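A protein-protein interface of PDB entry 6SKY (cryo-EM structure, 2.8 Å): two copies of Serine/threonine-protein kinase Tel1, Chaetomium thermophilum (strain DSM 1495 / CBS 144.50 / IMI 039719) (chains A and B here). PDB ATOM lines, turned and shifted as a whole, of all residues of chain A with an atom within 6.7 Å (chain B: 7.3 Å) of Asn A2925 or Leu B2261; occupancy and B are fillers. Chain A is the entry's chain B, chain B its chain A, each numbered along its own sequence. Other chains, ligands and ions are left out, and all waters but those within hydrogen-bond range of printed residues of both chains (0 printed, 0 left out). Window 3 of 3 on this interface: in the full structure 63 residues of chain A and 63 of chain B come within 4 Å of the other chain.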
ATOM      1  N   LEU A2800      -3.063  16.512   2.349  1.00  0.00           N
ATOM      2  CA  LEU A2800      -2.266  16.456   1.132  1.00  0.00           C
ATOM      3  C   LEU A2800      -3.150  16.741  -0.071  1.00  0.00           C
ATOM      4  O   LEU A2800      -3.187  15.979  -1.034  1.00  0.00           O
ATOM      5  CB  LEU A2800      -1.571  15.109   0.994  1.00  0.00           C
ATOM      6  CG  LEU A2800      -0.292  15.019   0.177  1.00  0.00           C
ATOM      7  CD1 LEU A2800       0.757  15.907   0.763  1.00  0.00           C
ATOM      8  CD2 LEU A2800       0.188  13.598   0.165  1.00  0.00           C
ATOM      9  N   ARG A2818       8.744  12.703  -0.579  1.00  0.00           N
ATOM     10  CA  ARG A2818       8.697  11.287  -0.248  1.00  0.00           C
ATOM     11  C   ARG A2818       9.949  10.844   0.496  1.00  0.00           C
ATOM     12  O   ARG A2818       9.866  10.066   1.452  1.00  0.00           O
ATOM     13  CB  ARG A2818       8.505  10.484  -1.520  1.00  0.00           C
ATOM     14  CG  ARG A2818       7.942   9.130  -1.300  1.00  0.00           C
ATOM     15  CD  ARG A2818       7.688   8.444  -2.605  1.00  0.00           C
ATOM     16  NE  ARG A2818       6.572   9.041  -3.321  1.00  0.00           N
ATOM     17  CZ  ARG A2818       5.340   8.558  -3.309  1.00  0.00           C
ATOM     18  NH1 ARG A2818       4.388   9.163  -3.990  1.00  0.00           N
ATOM     19  NH2 ARG A2818       5.065   7.469  -2.618  1.00  0.00           N
ATOM     20  N   MET A2917       9.382   2.431   3.119  1.00  0.00           N
ATOM     21  CA  MET A2917       8.925   2.736   1.768  1.00  0.00           C
ATOM     22  C   MET A2917       7.471   2.337   1.572  1.00  0.00           C
ATOM     23  O   MET A2917       6.666   3.123   1.068  1.00  0.00           O
ATOM     24  CB  MET A2917       9.811   2.025   0.751  1.00  0.00           C
ATOM     25  CG  MET A2917       9.445   2.325  -0.686  1.00  0.00           C
ATOM     26  SD  MET A2917       9.936   1.064  -1.875  1.00  0.00           S
ATOM     27  CE  MET A2917       8.927  -0.310  -1.351  1.00  0.00           C
ATOM     28  N   ALA A2918       7.115   1.115   1.961  1.00  0.00           N
ATOM     29  CA  ALA A2918       5.753   0.639   1.766  1.00  0.00           C
ATOM     30  C   ALA A2918       4.763   1.408   2.627  1.00  0.00           C
ATOM     31  O   ALA A2918       3.649   1.713   2.185  1.00  0.00           O
ATOM     32  CB  ALA A2918       5.680  -0.849   2.074  1.00  0.00           C
ATOM     33  N   VAL A2920       5.047   4.576   3.723  1.00  0.00           N
ATOM     34  CA  VAL A2920       4.867   5.904   3.153  1.00  0.00           C
ATOM     35  C   VAL A2920       4.062   5.837   1.863  1.00  0.00           C
ATOM     36  O   VAL A2920       3.249   6.721   1.586  1.00  0.00           O
ATOM     37  CB  VAL A2920       6.233   6.577   2.946  1.00  0.00           C
ATOM     38  CG1 VAL A2920       6.079   7.886   2.233  1.00  0.00           C
ATOM     39  CG2 VAL A2920       6.893   6.799   4.269  1.00  0.00           C
ATOM     40  N   ASN A2921       4.257   4.792   1.057  1.00  0.00           N
ATOM     41  CA  ASN A2921       3.445   4.635  -0.144  1.00  0.00           C
ATOM     42  C   ASN A2921       1.974   4.523   0.204  1.00  0.00           C
ATOM     43  O   ASN A2921       1.128   5.172  -0.415  1.00  0.00           O
ATOM     44  CB  ASN A2921       3.883   3.406  -0.932  1.00  0.00           C
ATOM     45  CG  ASN A2921       5.171   3.610  -1.657  1.00  0.00           C
ATOM     46  OD1 ASN A2921       5.851   4.603  -1.459  1.00  0.00           O
ATOM     47  ND2 ASN A2921       5.529   2.660  -2.496  1.00  0.00           N
ATOM     48  N   ASP A2922       1.649   3.698   1.195  1.00  0.00           N
ATOM     49  CA  ASP A2922       0.251   3.536   1.574  1.00  0.00           C
ATOM     50  C   ASP A2922      -0.330   4.828   2.131  1.00  0.00           C
ATOM     51  O   ASP A2922      -1.480   5.180   1.840  1.00  0.00           O
ATOM     52  CB  ASP A2922       0.120   2.408   2.586  1.00  0.00           C
ATOM     53  CG  ASP A2922      -1.113   1.565   2.357  1.00  0.00           C
ATOM     54  OD1 ASP A2922      -1.761   1.729   1.301  1.00  0.00           O
ATOM     55  OD2 ASP A2922      -1.442   0.735   3.230  1.00  0.00           O
ATOM     56  N   LEU A2923       0.456   5.559   2.924  1.00  0.00           N
ATOM     57  CA  LEU A2923      -0.024   6.810   3.499  1.00  0.00           C
ATOM     58  C   LEU A2923      -0.300   7.849   2.426  1.00  0.00           C
ATOM     59  O   LEU A2923      -1.323   8.532   2.464  1.00  0.00           O
ATOM     60  CB  LEU A2923       0.984   7.348   4.503  1.00  0.00           C
ATOM     61  CG  LEU A2923       1.107   6.597   5.814  1.00  0.00           C
ATOM     62  CD1 LEU A2923       2.209   7.192   6.620  1.00  0.00           C
ATOM     63  CD2 LEU A2923      -0.190   6.667   6.540  1.00  0.00           C
ATOM     64  N   ILE A2924       0.613   8.001   1.467  1.00  0.00           N
ATOM     65  CA  ILE A2924       0.402   8.983   0.413  1.00  0.00           C
ATOM     66  C   ILE A2924      -0.702   8.535  -0.528  1.00  0.00           C
ATOM     67  O   ILE A2924      -1.361   9.364  -1.156  1.00  0.00           O
ATOM     68  CB  ILE A2924       1.718   9.259  -0.334  1.00  0.00           C
ATOM     69  CG1 ILE A2924       2.770   9.789   0.625  1.00  0.00           C
ATOM     70  CG2 ILE A2924       1.526  10.271  -1.414  1.00  0.00           C
ATOM     71  CD1 ILE A2924       4.014  10.244  -0.039  1.00  0.00           C
ATOM     72  N   ASN A2925      -0.948   7.232  -0.639  1.00  0.00           N
ATOM     73  CA  ASN A2925      -2.083   6.784  -1.437  1.00  0.00           C
ATOM     74  C   ASN A2925      -3.398   7.147  -0.776  1.00  0.00           C
ATOM     75  O   ASN A2925      -4.325   7.606  -1.445  1.00  0.00           O
ATOM     76  CB  ASN A2925      -2.023   5.279  -1.662  1.00  0.00           C
ATOM     77  CG  ASN A2925      -1.143   4.896  -2.814  1.00  0.00           C
ATOM     78  OD1 ASN A2925      -0.476   3.871  -2.774  1.00  0.00           O
ATOM     79  ND2 ASN A2925      -1.136   5.712  -3.852  1.00  0.00           N
ATOM     80  N   GLN A2926      -3.513   6.928   0.530  1.00  0.00           N
ATOM     81  CA  GLN A2926      -4.788   7.207   1.172  1.00  0.00           C
ATOM     82  C   GLN A2926      -4.970   8.670   1.532  1.00  0.00           C
ATOM     83  O   GLN A2926      -6.092   9.075   1.833  1.00  0.00           O
ATOM     84  CB  GLN A2926      -4.974   6.334   2.412  1.00  0.00           C
ATOM     85  CG  GLN A2926      -3.936   6.500   3.469  1.00  0.00           C
ATOM     86  CD  GLN A2926      -4.184   5.605   4.661  1.00  0.00           C
ATOM     87  OE1 GLN A2926      -4.848   5.998   5.617  1.00  0.00           O
ATOM     88  NE2 GLN A2926      -3.648   4.396   4.614  1.00  0.00           N
ATOM     89  N   ALA A2927      -3.918   9.479   1.478  1.00  0.00           N
ATOM     90  CA  ALA A2927      -4.067  10.901   1.734  1.00  0.00           C
ATOM     91  C   ALA A2927      -4.503  11.683   0.509  1.00  0.00           C
ATOM     92  O   ALA A2927      -5.083  12.757   0.662  1.00  0.00           O
ATOM     93  CB  ALA A2927      -2.762  11.481   2.261  1.00  0.00           C
ATOM     94  N   THR A2928      -4.230  11.183  -0.693  1.00  0.00           N
ATOM     95  CA  THR A2928      -4.571  11.865  -1.934  1.00  0.00           C
ATOM     96  C   THR A2928      -5.700  11.182  -2.688  1.00  0.00           C
ATOM     97  O   THR A2928      -5.991  11.568  -3.820  1.00  0.00           O
ATOM     98  CB  THR A2928      -3.347  11.969  -2.841  1.00  0.00           C
ATOM     99  OG1 THR A2928      -2.722  10.694  -2.952  1.00  0.00           O
ATOM    100  CG2 THR A2928      -2.348  12.944  -2.290  1.00  0.00           C
ATOM    101  N   SER A2929      -6.351  10.197  -2.085  1.00  0.00           N
ATOM    102  CA  SER A2929      -7.372   9.424  -2.772  1.00  0.00           C
ATOM    103  C   SER A2929      -8.653  10.226  -2.926  1.00  0.00           C
ATOM    104  O   SER A2929      -9.116  10.865  -1.984  1.00  0.00           O
ATOM    105  CB  SER A2929      -7.652   8.143  -1.998  1.00  0.00           C
ATOM    106  OG  SER A2929      -8.652   7.374  -2.624  1.00  0.00           O
ATOM    107  N   VAL A2930      -9.236  10.181  -4.123  1.00  0.00           N
ATOM    108  CA  VAL A2930     -10.450  10.945  -4.386  1.00  0.00           C
ATOM    109  C   VAL A2930     -11.642  10.348  -3.654  1.00  0.00           C
ATOM    110  O   VAL A2930     -12.591  11.059  -3.319  1.00  0.00           O
ATOM    111  CB  VAL A2930     -10.695  11.032  -5.901  1.00  0.00           C
ATOM    112  CG1 VAL A2930     -12.044  11.643  -6.197  1.00  0.00           C
ATOM    113  CG2 VAL A2930      -9.611  11.851  -6.549  1.00  0.00           C
ATOM    114  N   ASN A2932     -11.460   9.153  -0.644  1.00  0.00           N
ATOM    115  CA  ASN A2932     -11.329   9.574   0.743  1.00  0.00           C
ATOM    116  C   ASN A2932     -11.538  11.062   0.912  1.00  0.00           C
ATOM    117  O   ASN A2932     -12.050  11.493   1.945  1.00  0.00           O
ATOM    118  CB  ASN A2932      -9.950   9.219   1.287  1.00  0.00           C
ATOM    119  CG  ASN A2932      -9.723   7.750   1.358  1.00  0.00           C
ATOM    120  OD1 ASN A2932     -10.554   6.964   0.922  1.00  0.00           O
ATOM    121  ND2 ASN A2932      -8.589   7.356   1.903  1.00  0.00           N
ATOM    122  N   MET B2220      12.726  -2.284  -5.708  1.00  0.00           N
ATOM    123  CA  MET B2220      11.360  -2.700  -5.986  1.00  0.00           C
ATOM    124  C   MET B2220      10.724  -1.864  -7.085  1.00  0.00           C
ATOM    125  O   MET B2220      10.082  -2.402  -7.993  1.00  0.00           O
ATOM    126  CB  MET B2220      10.529  -2.621  -4.713  1.00  0.00           C
ATOM    127  CG  MET B2220      10.987  -3.557  -3.633  1.00  0.00           C
ATOM    128  SD  MET B2220       9.750  -3.726  -2.350  1.00  0.00           S
ATOM    129  CE  MET B2220      10.447  -5.069  -1.406  1.00  0.00           C
ATOM    130  N   ILE B2221      10.880  -0.545  -7.027  1.00  0.00           N
ATOM    131  CA  ILE B2221      10.189   0.284  -8.002  1.00  0.00           C
ATOM    132  C   ILE B2221      10.812   0.126  -9.375  1.00  0.00           C
ATOM    133  O   ILE B2221      10.105   0.143 -10.385  1.00  0.00           O
ATOM    134  CB  ILE B2221      10.168   1.751  -7.549  1.00  0.00           C
ATOM    135  CG1 ILE B2221       9.700   1.852  -6.102  1.00  0.00           C
ATOM    136  CG2 ILE B2221       9.232   2.547  -8.408  1.00  0.00           C
ATOM    137  CD1 ILE B2221       8.343   1.294  -5.864  1.00  0.00           C
ATOM    138  N   ILE B2224       9.398  -3.090 -10.819  1.00  0.00           N
ATOM    139  CA  ILE B2224       8.006  -2.940 -11.232  1.00  0.00           C
ATOM    140  C   ILE B2224       7.908  -2.144 -12.527  1.00  0.00           C
ATOM    141  O   ILE B2224       7.133  -2.492 -13.425  1.00  0.00           O
ATOM    142  CB  ILE B2224       7.191  -2.297 -10.102  1.00  0.00           C
ATOM    143  CG1 ILE B2224       7.137  -3.230  -8.903  1.00  0.00           C
ATOM    144  CG2 ILE B2224       5.807  -1.983 -10.566  1.00  0.00           C
ATOM    145  CD1 ILE B2224       6.635  -2.578  -7.663  1.00  0.00           C
ATOM    146  N   ARG B2225       8.687  -1.067 -12.649  1.00  0.00           N
ATOM    147  CA  ARG B2225       8.650  -0.267 -13.868  1.00  0.00           C
ATOM    148  C   ARG B2225       9.153  -1.059 -15.062  1.00  0.00           C
ATOM    149  O   ARG B2225       8.618  -0.939 -16.169  1.00  0.00           O
ATOM    150  CB  ARG B2225       9.475   0.998 -13.694  1.00  0.00           C
ATOM    151  CG  ARG B2225       9.010   1.919 -12.606  1.00  0.00           C
ATOM    152  CD  ARG B2225       7.535   2.182 -12.679  1.00  0.00           C
ATOM    153  NE  ARG B2225       7.110   3.056 -11.593  1.00  0.00           N
ATOM    154  CZ  ARG B2225       5.854   3.198 -11.196  1.00  0.00           C
ATOM    155  NH1 ARG B2225       5.561   4.020 -10.203  1.00  0.00           N
ATOM    156  NH2 ARG B2225       4.891   2.518 -11.788  1.00  0.00           N
ATOM    157  N   GLN B2228       6.397  -3.499 -16.102  1.00  0.00           N
ATOM    158  CA  GLN B2228       5.320  -2.793 -16.784  1.00  0.00           C
ATOM    159  C   GLN B2228       5.729  -2.359 -18.180  1.00  0.00           C
ATOM    160  O   GLN B2228       4.889  -2.312 -19.080  1.00  0.00           O
ATOM    161  CB  GLN B2228       4.886  -1.589 -15.969  1.00  0.00           C
ATOM    162  CG  GLN B2228       4.116  -1.936 -14.735  1.00  0.00           C
ATOM    163  CD  GLN B2228       3.927  -0.759 -13.840  1.00  0.00           C
ATOM    164  OE1 GLN B2228       4.648   0.221 -13.938  1.00  0.00           O
ATOM    165  NE2 GLN B2228       2.950  -0.837 -12.964  1.00  0.00           N
ATOM    166  N   GLN B2255       4.161  -7.920  -7.140  1.00  0.00           N
ATOM    167  CA  GLN B2255       5.181  -6.959  -6.748  1.00  0.00           C
ATOM    168  C   GLN B2255       4.586  -5.605  -6.398  1.00  0.00           C
ATOM    169  O   GLN B2255       5.102  -4.921  -5.515  1.00  0.00           O
ATOM    170  CB  GLN B2255       6.216  -6.828  -7.852  1.00  0.00           C
ATOM    171  CG  GLN B2255       7.021  -8.071  -8.029  1.00  0.00           C
ATOM    172  CD  GLN B2255       8.154  -7.893  -8.975  1.00  0.00           C
ATOM    173  OE1 GLN B2255       8.926  -8.808  -9.210  1.00  0.00           O
ATOM    174  NE2 GLN B2255       8.267  -6.716  -9.531  1.00  0.00           N
ATOM    175  N   VAL B2256       3.505  -5.200  -7.062  1.00  0.00           N
ATOM    176  CA  VAL B2256       2.850  -3.946  -6.717  1.00  0.00           C
ATOM    177  C   VAL B2256       2.150  -4.054  -5.371  1.00  0.00           C
ATOM    178  O   VAL B2256       2.074  -3.073  -4.630  1.00  0.00           O
ATOM    179  CB  VAL B2256       1.877  -3.540  -7.837  1.00  0.00           C
ATOM    180  CG1 VAL B2256       0.988  -2.430  -7.396  1.00  0.00           C
ATOM    181  CG2 VAL B2256       2.634  -3.103  -9.043  1.00  0.00           C
ATOM    182  N   SER B2257       1.636  -5.233  -5.020  1.00  0.00           N
ATOM    183  CA  SER B2257       1.032  -5.396  -3.702  1.00  0.00           C
ATOM    184  C   SER B2257       2.074  -5.371  -2.599  1.00  0.00           C
ATOM    185  O   SER B2257       1.828  -4.820  -1.525  1.00  0.00           O
ATOM    186  CB  SER B2257       0.248  -6.698  -3.631  1.00  0.00           C
ATOM    187  OG  SER B2257      -0.740  -6.750  -4.634  1.00  0.00           O
ATOM    188  N   VAL B2258       3.232  -5.988  -2.825  1.00  0.00           N
ATOM    189  CA  VAL B2258       4.262  -6.012  -1.791  1.00  0.00           C
ATOM    190  C   VAL B2258       4.786  -4.612  -1.512  1.00  0.00           C
ATOM    191  O   VAL B2258       5.040  -4.252  -0.360  1.00  0.00           O
ATOM    192  CB  VAL B2258       5.397  -6.970  -2.191  1.00  0.00           C
ATOM    193  CG1 VAL B2258       6.610  -6.746  -1.339  1.00  0.00           C
ATOM    194  CG2 VAL B2258       4.941  -8.380  -2.060  1.00  0.00           C
ATOM    195  N   ALA B2259       4.959  -3.803  -2.547  1.00  0.00           N
ATOM    196  CA  ALA B2259       5.493  -2.458  -2.405  1.00  0.00           C
ATOM    197  C   ALA B2259       4.436  -1.423  -2.064  1.00  0.00           C
ATOM    198  O   ALA B2259       4.785  -0.262  -1.856  1.00  0.00           O
ATOM    199  CB  ALA B2259       6.208  -2.038  -3.686  1.00  0.00           C
ATOM    200  N   ARG B2260       3.165  -1.813  -1.995  1.00  0.00           N
ATOM    201  CA  ARG B2260       2.057  -0.907  -1.705  1.00  0.00           C
ATOM    202  C   ARG B2260       1.986   0.233  -2.704  1.00  0.00           C
ATOM    203  O   ARG B2260       1.525   1.322  -2.381  1.00  0.00           O
ATOM    204  CB  ARG B2260       2.142  -0.344  -0.292  1.00  0.00           C
ATOM    205  CG  ARG B2260       2.228  -1.368   0.789  1.00  0.00           C
ATOM    206  CD  ARG B2260       0.968  -2.141   0.872  1.00  0.00           C
ATOM    207  NE  ARG B2260       0.977  -3.037   2.014  1.00  0.00           N
ATOM    208  CZ  ARG B2260       0.410  -2.753   3.176  1.00  0.00           C
ATOM    209  NH1 ARG B2260       0.460  -3.624   4.171  1.00  0.00           N
ATOM    210  NH2 ARG B2260      -0.211  -1.598   3.340  1.00  0.00           N
ATOM    211  N   LEU B2261       2.436  -0.012  -3.928  1.00  0.00           N
ATOM    212  CA  LEU B2261       2.574   1.056  -4.900  1.00  0.00           C
ATOM    213  C   LEU B2261       1.236   1.558  -5.408  1.00  0.00           C
ATOM    214  O   LEU B2261       1.173   2.661  -5.951  1.00  0.00           O
ATOM    215  CB  LEU B2261       3.424   0.574  -6.066  1.00  0.00           C
ATOM    216  CG  LEU B2261       4.079   1.642  -6.918  1.00  0.00           C
ATOM    217  CD1 LEU B2261       4.939   2.499  -6.044  1.00  0.00           C
ATOM    218  CD2 LEU B2261       4.900   0.991  -7.979  1.00  0.00           C
ATOM    219  N   GLU B2262       0.172   0.781  -5.256  1.00  0.00           N
ATOM    220  CA  GLU B2262      -1.153   1.192  -5.683  1.00  0.00           C
ATOM    221  C   GLU B2262      -2.167   0.680  -4.681  1.00  0.00           C
ATOM    222  O   GLU B2262      -1.884  -0.217  -3.887  1.00  0.00           O
ATOM    223  CB  GLU B2262      -1.490   0.674  -7.076  1.00  0.00           C
ATOM    224  CG  GLU B2262      -0.614   1.255  -8.155  1.00  0.00           C
ATOM    225  CD  GLU B2262      -0.802   0.582  -9.481  1.00  0.00           C
ATOM    226  OE1 GLU B2262      -1.854  -0.053  -9.670  1.00  0.00           O
ATOM    227  OE2 GLU B2262       0.104   0.683 -10.331  1.00  0.00           O
ATOM    228  N   SER B2263      -3.353   1.261  -4.721  1.00  0.00           N
ATOM    229  CA  SER B2263      -4.383   0.865  -3.784  1.00  0.00           C
ATOM    230  C   SER B2263      -4.902  -0.522  -4.144  1.00  0.00           C
ATOM    231  O   SER B2263      -5.008  -0.854  -5.323  1.00  0.00           O
ATOM    232  CB  SER B2263      -5.531   1.863  -3.791  1.00  0.00           C
ATOM    233  OG  SER B2263      -6.374   1.648  -4.904  1.00  0.00           O
ATOM    234  N   PRO B2264      -5.253  -1.338  -3.157  1.00  0.00           N
ATOM    235  CA  PRO B2264      -5.695  -2.708  -3.441  1.00  0.00           C
ATOM    236  C   PRO B2264      -6.942  -2.814  -4.300  1.00  0.00           C
ATOM    237  O   PRO B2264      -7.352  -3.918  -4.654  1.00  0.00           O
ATOM    238  CB  PRO B2264      -5.943  -3.278  -2.043  1.00  0.00           C
ATOM    239  CG  PRO B2264      -6.075  -2.119  -1.172  1.00  0.00           C
ATOM    240  CD  PRO B2264      -5.171  -1.092  -1.715  1.00  0.00           C
ATOM    241  N   ILE B2267      -5.140  -2.709  -7.927  1.00  0.00           N
ATOM    242  CA  ILE B2267      -4.391  -3.933  -8.180  1.00  0.00           C
ATOM    243  C   ILE B2267      -5.306  -5.003  -8.743  1.00  0.00           C
ATOM    244  O   ILE B2267      -4.950  -5.705  -9.689  1.00  0.00           O
ATOM    245  CB  ILE B2267      -3.693  -4.412  -6.899  1.00  0.00           C
ATOM    246  CG1 ILE B2267      -2.687  -3.381  -6.426  1.00  0.00           C
ATOM    247  CG2 ILE B2267      -2.981  -5.702  -7.147  1.00  0.00           C
ATOM    248  CD1 ILE B2267      -2.057  -3.731  -5.133  1.00  0.00           C
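The side-chain amide nitrogen (ND2) of Asn A2921 is in hydrogen-bond range of the backbone carbonyl oxygen (O) of Ala B2259 (3.1 Å).
The backbone carbonyl oxygen (O) of Arg B2260 lies close to the side-chain amide oxygen (OD1) of Asn A2925.
OD2 of Asp A2922 is in salt-bridge range of NH2 of Arg B2260 (2.6 Å).
N of Leu B2261 sits at hydrogen-bond distance from O of Val B2256.
The backbone carbonyl oxygen (O) of Met A2917 lies close to the side-chain amide oxygen (OD1) of Asn A2921 (3.0 Å).
The guanidinium group (NH2) of Arg A2818 is in hydrogen-bond range of the side-chain amide oxygen (OD1) of Asn A2921, 3.2 Å away.
O of Asn A2921 sits close to OD1 of Asn A2925 (3.1 Å).
Met A2917 touches Met B2220 (CE to SD, 3.7 Å).
Ala B2259 touches Met A2917 (CB to CE, 3.98 Å).
Ala B2259 touches Ala A2918 (O to CA, 3.9 Å).
Arg B2260 touches Ala A2918 (CB to O, 3.6 Å).
Arg B2260 touches Asn A2921 (O to CB, 3.5 Å).
Leu B2261 touches Asn A2921.
Asn A2925 touches Leu B2261.
Of the printed residues of chain B, Met A2917 touches Met B2220 and Ala B2259.
Printed residues of chain B within 4 Å of Ala A2918: Ala B2259 and Arg B2260.
Of the printed residues of chain B, Asn A2921 touches Ala B2259, Arg B2260 and Leu B2261.
Printed residues of chain B within 4 Å of Asn A2925: Arg B2260 and Leu B2261.
Printed residues of chain A within 4 Å of Met B2220: Met A2917 (3.7 Å).
Of the printed residues of chain A, Arg B2260 touches Ala A2918 (3.6 Å), Asn A2921 (3.5 Å), Asp A2922 (2.6 Å) and Asn A2925 (3.3 Å).
Of the printed residues of chain A, Leu B2261 touches Asn A2921 and Asn A2925.
The nearest printed residue of chain B that does not touch Asn A2925 is Glu B2262 (4.01 Å).
The nearest residue of chain A that does not touch Leu B2261 is Arg A2818 (6.0 Å).
The nearest printed residue of chain B that does not touch Ala A2918 is Val B2258 (4.2 Å).
Hydrophobic or aromatic side chains of chain B within 4 Å of the printed part of chain A: Met B2220, Ala B2259 and Leu B2261.
Among the printed residues, 10 pairs touch across the chains.
No position is printed for both chains.
Of the 10 pairs that touch across the chains among the printed residues, none has its exchanged pair printed and touching as well.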
